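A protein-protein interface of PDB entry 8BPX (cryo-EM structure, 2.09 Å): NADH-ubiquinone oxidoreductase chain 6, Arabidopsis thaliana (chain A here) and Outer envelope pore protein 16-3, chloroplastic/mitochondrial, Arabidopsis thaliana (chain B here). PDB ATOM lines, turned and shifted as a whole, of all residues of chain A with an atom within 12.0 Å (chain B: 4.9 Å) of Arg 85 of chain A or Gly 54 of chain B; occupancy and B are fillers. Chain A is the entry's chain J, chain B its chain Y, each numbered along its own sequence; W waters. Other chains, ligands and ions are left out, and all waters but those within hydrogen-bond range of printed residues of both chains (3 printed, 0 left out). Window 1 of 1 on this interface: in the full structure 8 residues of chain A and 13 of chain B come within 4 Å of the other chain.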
ATOM      1  N   ARG A  19     -10.392  10.385  23.624  1.00  0.00           N
ATOM      2  CA  ARG A  19     -10.971   9.058  23.800  1.00  0.00           C
ATOM      3  C   ARG A  19     -12.495   9.012  23.823  1.00  0.00           C
ATOM      4  O   ARG A  19     -13.054   7.911  23.778  1.00  0.00           O
ATOM      5  CB  ARG A  19     -10.442   8.408  25.089  1.00  0.00           C
ATOM      6  CG  ARG A  19      -8.971   8.024  25.037  1.00  0.00           C
ATOM      7  CD  ARG A  19      -8.785   6.528  24.841  1.00  0.00           C
ATOM      8  NE  ARG A  19      -9.474   6.019  23.661  1.00  0.00           N
ATOM      9  CZ  ARG A  19     -10.551   5.245  23.699  1.00  0.00           C
ATOM     10  NH1 ARG A  19     -11.102   4.882  24.846  1.00  0.00           N
ATOM     11  NH2 ARG A  19     -11.086   4.823  22.557  1.00  0.00           N
ATOM     12  N   ILE A  79     -16.633   5.895  12.890  1.00  0.00           N
ATOM     13  CA  ILE A  79     -15.353   6.366  13.477  1.00  0.00           C
ATOM     14  C   ILE A  79     -14.970   5.454  14.656  1.00  0.00           C
ATOM     15  O   ILE A  79     -14.026   5.769  15.298  1.00  0.00           O
ATOM     16  CB  ILE A  79     -15.503   7.872  13.826  1.00  0.00           C
ATOM     17  CG1 ILE A  79     -16.752   8.046  14.698  1.00  0.00           C
ATOM     18  CG2 ILE A  79     -15.555   8.767  12.610  1.00  0.00           C
ATOM     19  CD1 ILE A  79     -16.673   9.115  15.746  1.00  0.00           C
ATOM     20  N   HIS A  80     -15.739   4.392  14.932  1.00  0.00           N
ATOM     21  CA  HIS A  80     -15.429   3.492  16.031  1.00  0.00           C
ATOM     22  C   HIS A  80     -14.237   2.601  15.705  1.00  0.00           C
ATOM     23  O   HIS A  80     -14.049   2.170  14.564  1.00  0.00           O
ATOM     24  CB  HIS A  80     -16.629   2.608  16.364  1.00  0.00           C
ATOM     25  CG  HIS A  80     -16.251   1.222  16.782  1.00  0.00           C
ATOM     26  ND1 HIS A  80     -15.964   0.893  18.090  1.00  0.00           N
ATOM     27  CD2 HIS A  80     -16.088   0.086  16.065  1.00  0.00           C
ATOM     28  CE1 HIS A  80     -15.649  -0.387  18.159  1.00  0.00           C
ATOM     29  NE2 HIS A  80     -15.717  -0.900  16.944  1.00  0.00           N
ATOM     30  N   GLU A  81     -13.515   2.306  16.769  1.00  0.00           N
ATOM     31  CA  GLU A  81     -12.435   1.288  16.662  1.00  0.00           C
ATOM     32  C   GLU A  81     -11.976   0.947  18.083  1.00  0.00           C
ATOM     33  O   GLU A  81     -11.919   1.853  18.885  1.00  0.00           O
ATOM     34  CB  GLU A  81     -11.256   1.723  15.803  1.00  0.00           C
ATOM     35  CG  GLU A  81      -9.941   1.095  16.154  1.00  0.00           C
ATOM     36  CD  GLU A  81      -8.809   1.719  15.384  1.00  0.00           C
ATOM     37  OE1 GLU A  81      -8.399   2.826  15.743  1.00  0.00           O
ATOM     38  OE2 GLU A  81      -8.384   1.113  14.412  1.00  0.00           O
ATOM     39  N   GLU A  82     -11.604  -0.290  18.316  1.00  0.00           N
ATOM     40  CA  GLU A  82     -11.049  -0.703  19.600  1.00  0.00           C
ATOM     41  C   GLU A  82      -9.610  -0.223  19.743  1.00  0.00           C
ATOM     42  O   GLU A  82      -8.810  -0.343  18.810  1.00  0.00           O
ATOM     43  CB  GLU A  82     -11.105  -2.221  19.731  1.00  0.00           C
ATOM     44  CG  GLU A  82     -12.369  -2.831  19.188  1.00  0.00           C
ATOM     45  CD  GLU A  82     -13.478  -2.846  20.210  1.00  0.00           C
ATOM     46  OE1 GLU A  82     -13.191  -2.606  21.401  1.00  0.00           O
ATOM     47  OE2 GLU A  82     -14.640  -3.090  19.826  1.00  0.00           O
ATOM     48  N   VAL A  83      -9.274   0.305  20.918  1.00  0.00           N
ATOM     49  CA  VAL A  83      -7.952   0.864  21.170  1.00  0.00           C
ATOM     50  C   VAL A  83      -7.121   0.012  22.114  1.00  0.00           C
ATOM     51  O   VAL A  83      -6.001   0.415  22.459  1.00  0.00           O
ATOM     52  CB  VAL A  83      -8.041   2.306  21.699  1.00  0.00           C
ATOM     53  CG1 VAL A  83      -8.725   3.208  20.683  1.00  0.00           C
ATOM     54  CG2 VAL A  83      -8.765   2.334  23.030  1.00  0.00           C
ATOM     55  N   LEU A  84      -7.625  -1.147  22.547  1.00  0.00           N
ATOM     56  CA  LEU A  84      -6.838  -2.006  23.428  1.00  0.00           C
ATOM     57  C   LEU A  84      -5.536  -2.440  22.767  1.00  0.00           C
ATOM     58  O   LEU A  84      -4.501  -2.538  23.435  1.00  0.00           O
ATOM     59  CB  LEU A  84      -7.661  -3.227  23.843  1.00  0.00           C
ATOM     60  CG  LEU A  84      -7.118  -4.172  24.923  1.00  0.00           C
ATOM     61  CD1 LEU A  84      -6.288  -3.429  25.946  1.00  0.00           C
ATOM     62  CD2 LEU A  84      -8.247  -4.937  25.599  1.00  0.00           C
ATOM     63  N   ARG A  85      -5.513  -2.698  21.469  1.00  0.00           N
ATOM     64  CA  ARG A  85      -4.333  -3.173  20.715  1.00  0.00           C
ATOM     65  C   ARG A  85      -3.289  -2.042  20.503  1.00  0.00           C
ATOM     66  O   ARG A  85      -2.275  -2.351  19.927  1.00  0.00           O
ATOM     67  CB  ARG A  85      -4.815  -3.756  19.391  1.00  0.00           C
ATOM     68  CG  ARG A  85      -5.364  -2.653  18.494  1.00  0.00           C
ATOM     69  CD  ARG A  85      -5.798  -2.910  17.071  1.00  0.00           C
ATOM     70  NE  ARG A  85      -4.671  -3.252  16.260  1.00  0.00           N
ATOM     71  CZ  ARG A  85      -4.438  -2.823  15.024  1.00  0.00           C
ATOM     72  NH1 ARG A  85      -5.290  -2.031  14.407  1.00  0.00           N
ATOM     73  NH2 ARG A  85      -3.352  -3.232  14.408  1.00  0.00           N
ATOM     74  N   TYR A  86      -3.598  -0.799  20.833  1.00  0.00           N
ATOM     75  CA  TYR A  86      -2.625   0.307  20.778  1.00  0.00           C
ATOM     76  C   TYR A  86      -1.850   0.500  22.092  1.00  0.00           C
ATOM     77  O   TYR A  86      -0.852   1.177  22.012  1.00  0.00           O
ATOM     78  CB  TYR A  86      -3.290   1.579  20.263  1.00  0.00           C
ATOM     79  CG  TYR A  86      -3.924   1.389  18.918  1.00  0.00           C
ATOM     80  CD1 TYR A  86      -3.151   1.258  17.782  1.00  0.00           C
ATOM     81  CD2 TYR A  86      -5.296   1.266  18.804  1.00  0.00           C
ATOM     82  CE1 TYR A  86      -3.734   1.062  16.541  1.00  0.00           C
ATOM     83  CE2 TYR A  86      -5.894   1.064  17.576  1.00  0.00           C
ATOM     84  CZ  TYR A  86      -5.107   0.948  16.447  1.00  0.00           C
ATOM     85  OH  TYR A  86      -5.695   0.725  15.249  1.00  0.00           O
ATOM     86  N   LEU A  87      -2.271  -0.099  23.213  1.00  0.00           N
ATOM     87  CA  LEU A  87      -1.566   0.104  24.477  1.00  0.00           C
ATOM     88  C   LEU A  87      -0.056  -0.093  24.387  1.00  0.00           C
ATOM     89  O   LEU A  87       0.674   0.719  24.979  1.00  0.00           O
ATOM     90  CB  LEU A  87      -2.154  -0.812  25.563  1.00  0.00           C
ATOM     91  CG  LEU A  87      -3.325  -0.260  26.373  1.00  0.00           C
ATOM     92  CD1 LEU A  87      -3.821  -1.292  27.371  1.00  0.00           C
ATOM     93  CD2 LEU A  87      -2.925   1.024  27.088  1.00  0.00           C
ATOM     94  N   PRO A  88       0.482  -1.115  23.709  1.00  0.00           N
ATOM     95  CA  PRO A  88       1.952  -1.208  23.622  1.00  0.00           C
ATOM     96  C   PRO A  88       2.591  -0.072  22.837  1.00  0.00           C
ATOM     97  O   PRO A  88       3.527   0.561  23.337  1.00  0.00           O
ATOM     98  CB  PRO A  88       2.188  -2.577  22.966  1.00  0.00           C
ATOM     99  CG  PRO A  88       0.882  -3.280  22.979  1.00  0.00           C
ATOM    100  CD  PRO A  88      -0.184  -2.257  23.056  1.00  0.00           C
ATOM    101  N   VAL A  89       2.105   0.219  21.625  1.00  0.00           N
ATOM    102  CA  VAL A  89       2.731   1.263  20.815  1.00  0.00           C
ATOM    103  C   VAL A  89       2.646   2.612  21.517  1.00  0.00           C
ATOM    104  O   VAL A  89       3.574   3.424  21.443  1.00  0.00           O
ATOM    105  CB  VAL A  89       2.115   1.310  19.401  1.00  0.00           C
ATOM    106  CG1 VAL A  89       0.694   1.860  19.426  1.00  0.00           C
ATOM    107  CG2 VAL A  89       2.985   2.143  18.481  1.00  0.00           C
ATOM    108  N   SER A  90       1.536   2.875  22.210  1.00  0.00           N
ATOM    109  CA  SER A  90       1.454   4.082  23.022  1.00  0.00           C
ATOM    110  C   SER A  90       2.378   3.998  24.228  1.00  0.00           C
ATOM    111  O   SER A  90       2.889   5.024  24.690  1.00  0.00           O
ATOM    112  CB  SER A  90       0.015   4.322  23.472  1.00  0.00           C
ATOM    113  OG  SER A  90      -0.447   3.248  24.271  1.00  0.00           O
ATOM    114  N   GLY A  91       2.596   2.790  24.752  1.00  0.00           N
ATOM    115  CA  GLY A  91       3.484   2.641  25.891  1.00  0.00           C
ATOM    116  C   GLY A  91       4.923   2.997  25.567  1.00  0.00           C
ATOM    117  O   GLY A  91       5.575   3.724  26.318  1.00  0.00           O
ATOM    118  N   ILE A  92       5.485   2.416  24.499  1.00  0.00           N
ATOM    119  CA  ILE A  92       6.872   2.817  24.115  1.00  0.00           C
ATOM    120  C   ILE A  92       6.858   4.314  23.766  1.00  0.00           C
ATOM    121  O   ILE A  92       7.569   5.077  24.440  1.00  0.00           O
ATOM    122  CB  ILE A  92       7.461   1.925  22.999  1.00  0.00           C
ATOM    123  CG1 ILE A  92       7.179   0.445  23.267  1.00  0.00           C
ATOM    124  CG2 ILE A  92       8.944   2.180  22.818  1.00  0.00           C
ATOM    125  CD1 ILE A  92       6.638  -0.305  22.078  1.00  0.00           C
ATOM    126  N   ILE A  93       6.058   4.726  22.787  1.00  0.00           N
ATOM    127  CA  ILE A  93       6.157   6.105  22.315  1.00  0.00           C
ATOM    128  C   ILE A  93       5.928   7.074  23.467  1.00  0.00           C
ATOM    129  O   ILE A  93       6.650   8.066  23.617  1.00  0.00           O
ATOM    130  CB  ILE A  93       5.174   6.356  21.158  1.00  0.00           C
ATOM    131  CG1 ILE A  93       5.508   5.465  19.959  1.00  0.00           C
ATOM    132  CG2 ILE A  93       5.223   7.808  20.737  1.00  0.00           C
ATOM    133  CD1 ILE A  93       6.753   5.863  19.219  1.00  0.00           C
ATOM    134  N   ALA B  38       2.582  -4.747  14.071  1.00  0.00           N
ATOM    135  CA  ALA B  38       1.215  -5.013  14.500  1.00  0.00           C
ATOM    136  C   ALA B  38       0.359  -3.756  14.421  1.00  0.00           C
ATOM    137  O   ALA B  38      -0.801  -3.814  14.001  1.00  0.00           O
ATOM    138  CB  ALA B  38       1.215  -5.581  15.919  1.00  0.00           C
ATOM    139  N   THR B  39       0.864  -2.607  14.784  1.00  0.00           N
ATOM    140  CA  THR B  39       0.081  -1.344  14.744  1.00  0.00           C
ATOM    141  C   THR B  39      -0.185  -0.912  13.272  1.00  0.00           C
ATOM    142  O   THR B  39      -1.225  -0.403  13.016  1.00  0.00           O
ATOM    143  CB  THR B  39       0.791  -0.283  15.584  1.00  0.00           C
ATOM    144  OG1 THR B  39       1.210  -0.841  16.829  1.00  0.00           O
ATOM    145  CG2 THR B  39      -0.051   0.951  15.819  1.00  0.00           C
ATOM    146  N   LYS B  41      -0.757  -2.727  10.571  1.00  0.00           N
ATOM    147  CA  LYS B  41      -1.827  -3.530   9.919  1.00  0.00           C
ATOM    148  C   LYS B  41      -3.222  -3.235  10.440  1.00  0.00           C
ATOM    149  O   LYS B  41      -3.382  -2.783  11.571  1.00  0.00           O
ATOM    150  CB  LYS B  41      -1.564  -5.027  10.074  1.00  0.00           C
ATOM    151  CG  LYS B  41      -0.092  -5.385  10.066  1.00  0.00           C
ATOM    152  CD  LYS B  41       0.185  -6.732  10.683  1.00  0.00           C
ATOM    153  CE  LYS B  41      -0.306  -7.868   9.816  1.00  0.00           C
ATOM    154  NZ  LYS B  41       0.248  -7.770   8.449  1.00  0.00           N
ATOM    155  N   ASP B  42      -4.184  -3.631   9.635  1.00  0.00           N
ATOM    156  CA  ASP B  42      -5.613  -3.448   9.985  1.00  0.00           C
ATOM    157  C   ASP B  42      -6.021  -4.639  10.836  1.00  0.00           C
ATOM    158  O   ASP B  42      -5.219  -5.588  10.902  1.00  0.00           O
ATOM    159  CB  ASP B  42      -6.445  -3.394   8.710  1.00  0.00           C
ATOM    160  CG  ASP B  42      -6.518  -4.740   8.021  1.00  0.00           C
ATOM    161  OD1 ASP B  42      -5.485  -5.174   7.479  1.00  0.00           O
ATOM    162  OD2 ASP B  42      -7.600  -5.355   8.063  1.00  0.00           O
ATOM    163  N   VAL B  43      -7.176  -4.580  11.472  1.00  0.00           N
ATOM    164  CA  VAL B  43      -7.716  -5.730  12.190  1.00  0.00           C
ATOM    165  C   VAL B  43      -8.653  -6.492  11.261  1.00  0.00           C
ATOM    166  O   VAL B  43      -9.280  -5.885  10.382  1.00  0.00           O
ATOM    167  CB  VAL B  43      -8.444  -5.304  13.475  1.00  0.00           C
ATOM    168  CG1 VAL B  43      -7.447  -5.104  14.609  1.00  0.00           C
ATOM    169  CG2 VAL B  43      -9.254  -4.042  13.232  1.00  0.00           C
ATOM    170  N   GLU B  47     -13.203  -8.955  13.778  1.00  0.00           N
ATOM    171  CA  GLU B  47     -12.622  -8.545  15.051  1.00  0.00           C
ATOM    172  C   GLU B  47     -12.784  -7.050  15.294  1.00  0.00           C
ATOM    173  O   GLU B  47     -12.129  -6.496  16.181  1.00  0.00           O
ATOM    174  CB  GLU B  47     -11.145  -8.936  15.112  1.00  0.00           C
ATOM    175  CG  GLU B  47     -10.917 -10.430  15.020  1.00  0.00           C
ATOM    176  CD  GLU B  47      -9.560 -10.842  15.539  1.00  0.00           C
ATOM    177  OE1 GLU B  47      -8.951 -11.758  14.949  1.00  0.00           O
ATOM    178  OE2 GLU B  47      -9.093 -10.240  16.525  1.00  0.00           O
ATOM    179  N   ALA B  51     -12.191  -6.225  21.367  1.00  0.00           N
ATOM    180  CA  ALA B  51     -10.897  -5.607  21.629  1.00  0.00           C
ATOM    181  C   ALA B  51      -9.798  -6.612  21.959  1.00  0.00           C
ATOM    182  O   ALA B  51      -8.673  -6.473  21.466  1.00  0.00           O
ATOM    183  CB  ALA B  51     -11.023  -4.603  22.774  1.00  0.00           C
ATOM    184  N   LEU B  52     -10.097  -7.607  22.796  1.00  0.00           N
ATOM    185  CA  LEU B  52      -9.044  -8.452  23.360  1.00  0.00           C
ATOM    186  C   LEU B  52      -8.213  -9.185  22.311  1.00  0.00           C
ATOM    187  O   LEU B  52      -6.974  -9.126  22.396  1.00  0.00           O
ATOM    188  CB  LEU B  52      -9.660  -9.429  24.368  1.00  0.00           C
ATOM    189  CG  LEU B  52      -8.719 -10.313  25.195  1.00  0.00           C
ATOM    190  CD1 LEU B  52      -7.448  -9.576  25.593  1.00  0.00           C
ATOM    191  CD2 LEU B  52      -9.433 -10.850  26.426  1.00  0.00           C
ATOM    192  N   PRO B  53      -8.792  -9.883  21.326  1.00  0.00           N
ATOM    193  CA  PRO B  53      -7.942 -10.637  20.384  1.00  0.00           C
ATOM    194  C   PRO B  53      -6.977  -9.774  19.593  1.00  0.00           C
ATOM    195  O   PRO B  53      -5.914 -10.265  19.205  1.00  0.00           O
ATOM    196  CB  PRO B  53      -8.957 -11.328  19.464  1.00  0.00           C
ATOM    197  CG  PRO B  53     -10.207 -10.578  19.641  1.00  0.00           C
ATOM    198  CD  PRO B  53     -10.220 -10.132  21.058  1.00  0.00           C
ATOM    199  N   GLY B  54      -7.316  -8.512  19.320  1.00  0.00           N
ATOM    200  CA  GLY B  54      -6.356  -7.635  18.669  1.00  0.00           C
ATOM    201  C   GLY B  54      -5.126  -7.397  19.520  1.00  0.00           C
ATOM    202  O   GLY B  54      -3.993  -7.469  19.034  1.00  0.00           O
ATOM    203  N   LEU B  55      -5.332  -7.135  20.812  1.00  0.00           N
ATOM    204  CA  LEU B  55      -4.212  -7.023  21.738  1.00  0.00           C
ATOM    205  C   LEU B  55      -3.429  -8.326  21.808  1.00  0.00           C
ATOM    206  O   LEU B  55      -2.193  -8.315  21.848  1.00  0.00           O
ATOM    207  CB  LEU B  55      -4.723  -6.625  23.123  1.00  0.00           C
ATOM    208  CG  LEU B  55      -3.712  -6.659  24.270  1.00  0.00           C
ATOM    209  CD1 LEU B  55      -2.875  -5.393  24.281  1.00  0.00           C
ATOM    210  CD2 LEU B  55      -4.422  -6.849  25.595  1.00  0.00           C
ATOM    211  N   ILE B  56      -4.135  -9.460  21.817  1.00  0.00           N
ATOM    212  CA  ILE B  56      -3.465 -10.757  21.884  1.00  0.00           C
ATOM    213  C   ILE B  56      -2.587 -10.969  20.657  1.00  0.00           C
ATOM    214  O   ILE B  56      -1.441 -11.417  20.762  1.00  0.00           O
ATOM    215  CB  ILE B  56      -4.497 -11.890  22.037  1.00  0.00           C
ATOM    216  CG1 ILE B  56      -5.257 -11.754  23.359  1.00  0.00           C
ATOM    217  CG2 ILE B  56      -3.814 -13.238  21.956  1.00  0.00           C
ATOM    218  CD1 ILE B  56      -4.372 -11.502  24.549  1.00  0.00           C
ATOM    219  N   ARG B  57      -3.116 -10.656  19.473  1.00  0.00           N
ATOM    220  CA  ARG B  57      -2.343 -10.815  18.246  1.00  0.00           C
ATOM    221  C   ARG B  57      -1.143  -9.878  18.220  1.00  0.00           C
ATOM    222  O   ARG B  57      -0.055 -10.264  17.775  1.00  0.00           O
ATOM    223  CB  ARG B  57      -3.241 -10.595  17.026  1.00  0.00           C
ATOM    224  CG  ARG B  57      -2.515 -10.048  15.810  1.00  0.00           C
ATOM    225  CD  ARG B  57      -3.443  -9.543  14.703  1.00  0.00           C
ATOM    226  NE  ARG B  57      -4.570 -10.430  14.428  1.00  0.00           N
ATOM    227  CZ  ARG B  57      -5.761 -10.358  15.008  1.00  0.00           C
ATOM    228  NH1 ARG B  57      -6.046  -9.418  15.891  1.00  0.00           N
ATOM    229  NH2 ARG B  57      -6.689 -11.254  14.687  1.00  0.00           N
ATOM    230  N   THR B  58      -1.319  -8.645  18.701  1.00  0.00           N
ATOM    231  CA  THR B  58      -0.196  -7.715  18.769  1.00  0.00           C
ATOM    232  C   THR B  58       0.897  -8.244  19.690  1.00  0.00           C
ATOM    233  O   THR B  58       2.085  -8.206  19.350  1.00  0.00           O
ATOM    234  CB  THR B  58      -0.681  -6.342  19.239  1.00  0.00           C
ATOM    235  OG1 THR B  58      -1.383  -5.690  18.175  1.00  0.00           O
ATOM    236  CG2 THR B  58       0.493  -5.475  19.665  1.00  0.00           C
HETATM  237  O   HOH W   1       0.169  -1.378  19.785  1.00  0.00           O
HETATM  238  O   HOH W   2      -7.788  -3.502  20.605  1.00  0.00           O
HETATM  239  O   HOH W   3      -1.197  -2.929  17.408  1.00  0.00           O
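The guanidinium group of Arg 85 of chain A lies within hydrogen-bond range of the backbone carbonyl oxygen of Ala 38 of chain B (2.6 Å).
NH2 of Arg 85 of chain A lies within hydrogen-bond range of O of Lys 41 of chain B (2.9 Å).
The guanidinium group of Arg 85 of chain A sits at hydrogen-bond distance from the side-chain hydroxyl of Tyr 86 of chain A (2.9 Å).
The backbone carbonyl oxygen (O) of Gly 54 of chain B is in hydrogen-bond range of the side-chain hydroxyl (OG1) of Thr 58 of chain B, at 3.3 Å.
OG of Ser 90 of chain A is in hydrogen-bond range of O of Tyr 86 of chain A (3.1 Å).
The side-chain hydroxyl (OH) of Tyr 86 of chain A sits at hydrogen-bond distance from the side-chain carboxylate (OE2) of Glu 81 of chain A (2.8 Å).
Among the printed residues, merely in contact across the chains: Glu 82 of chain A with Ala 51 of chain B (3.3 Å), Leu 84 of chain A with Leu 55 of chain B (3.4 Å), Val 89 of chain A with Thr 39 of chain B (3.5 Å), Arg 85 of chain A with Gly 54 of chain B (3.7 Å), Tyr 86 of chain A with Thr 39 of chain B (3.7 Å), Arg 85 of chain A with Val 43 of chain B (3.7 Å), Arg 85 of chain A with Leu 55 of chain B (3.7 Å), Leu 84 of chain A with Ala 51 of chain B (3.8 Å), Arg 85 of chain A with Thr 39 of chain B (3.8 Å), Arg 85 of chain A with Thr 58 of chain B (3.9 Å) and Pro 88 of chain A with Thr 58 of chain B (3.99 Å).
Of the printed residues of chain B, Arg 85 of chain A touches Ala 38 (2.6 Å), Thr 39 (3.8 Å), Lys 41 (2.9 Å), Val 43 (3.7 Å), Gly 54 (3.7 Å), Leu 55 (3.7 Å) and Thr 58 (3.9 Å).
No residue of chain A comes within 4 Å of Asp 42 of chain B.
Val 43 of chain B touches just one residue of chain A: Arg 85 (3.7 Å).
Ala 51 of chain B touches just these residues of chain A: Glu 82 and Leu 84.
No residue of chain A comes within 4 Å of Leu 52 of chain B.
No residue of chain A comes within 4 Å of Pro 53 of chain B.
Of chain A, only Leu 84 and Arg 85 come within 4 Å of Leu 55 of chain B.
No residue of chain A comes within 4 Å of Ile 56 of chain B.
No residue of chain A comes within 4 Å of Arg 57 of chain B.
Of the printed residues of chain A, Lys 41 of chain B touches Arg 85.
Of the printed residues of chain B, Tyr 86 of chain A touches Thr 39 (3.7 Å).
Of the printed residues of chain B, Val 89 of chain A touches Thr 39 (3.5 Å).
Of the printed residues of chain A, Thr 58 of chain B touches Arg 85 (3.9 Å) and Pro 88 (3.99 Å).
Printed residues of chain B within 4 Å of Leu 84 of chain A: Ala 51 and Leu 55.
Leu 87 of chain A touches none of the printed residues of chain B.
The nearest residue of chain B that does not touch Arg 85 of chain A is Asp 42 of chain B (4.5 Å).
The nearest residue of chain A that does not touch Gly 54 of chain B is Leu 84 of chain A (5.9 Å).
The nearest printed residue of chain B that does not touch Tyr 86 of chain A is Lys 41 of chain B (5.6 Å).
Hydrophobic or aromatic side chains of chain B within 4 Å of the printed part of chain A: Val 43, Ala 51 and Leu 55.
Among the printed residues, 13 pairs touch across the chains.
Water W2 lies within hydrogen-bond range of the backbone NH (N) of Arg 85 of chain A (2.6 Å), the backbone NH (N) of Leu 84 of chain A (3.1 Å) and the backbone carbonyl oxygen (O) of Ala 51 of chain B (3.2 Å).
Water W1 lies within hydrogen-bond range of O of Arg 85 of chain A (2.6 Å), N of Val 89 of chain A (3.1 Å) and OG1 of Thr 39 of chain B (3.2 Å).
Water W3 lies within hydrogen-bond range of O of Arg 85 of chain A, OG1 of Thr 58 of chain B and OG1 of Thr 39 of chain B.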
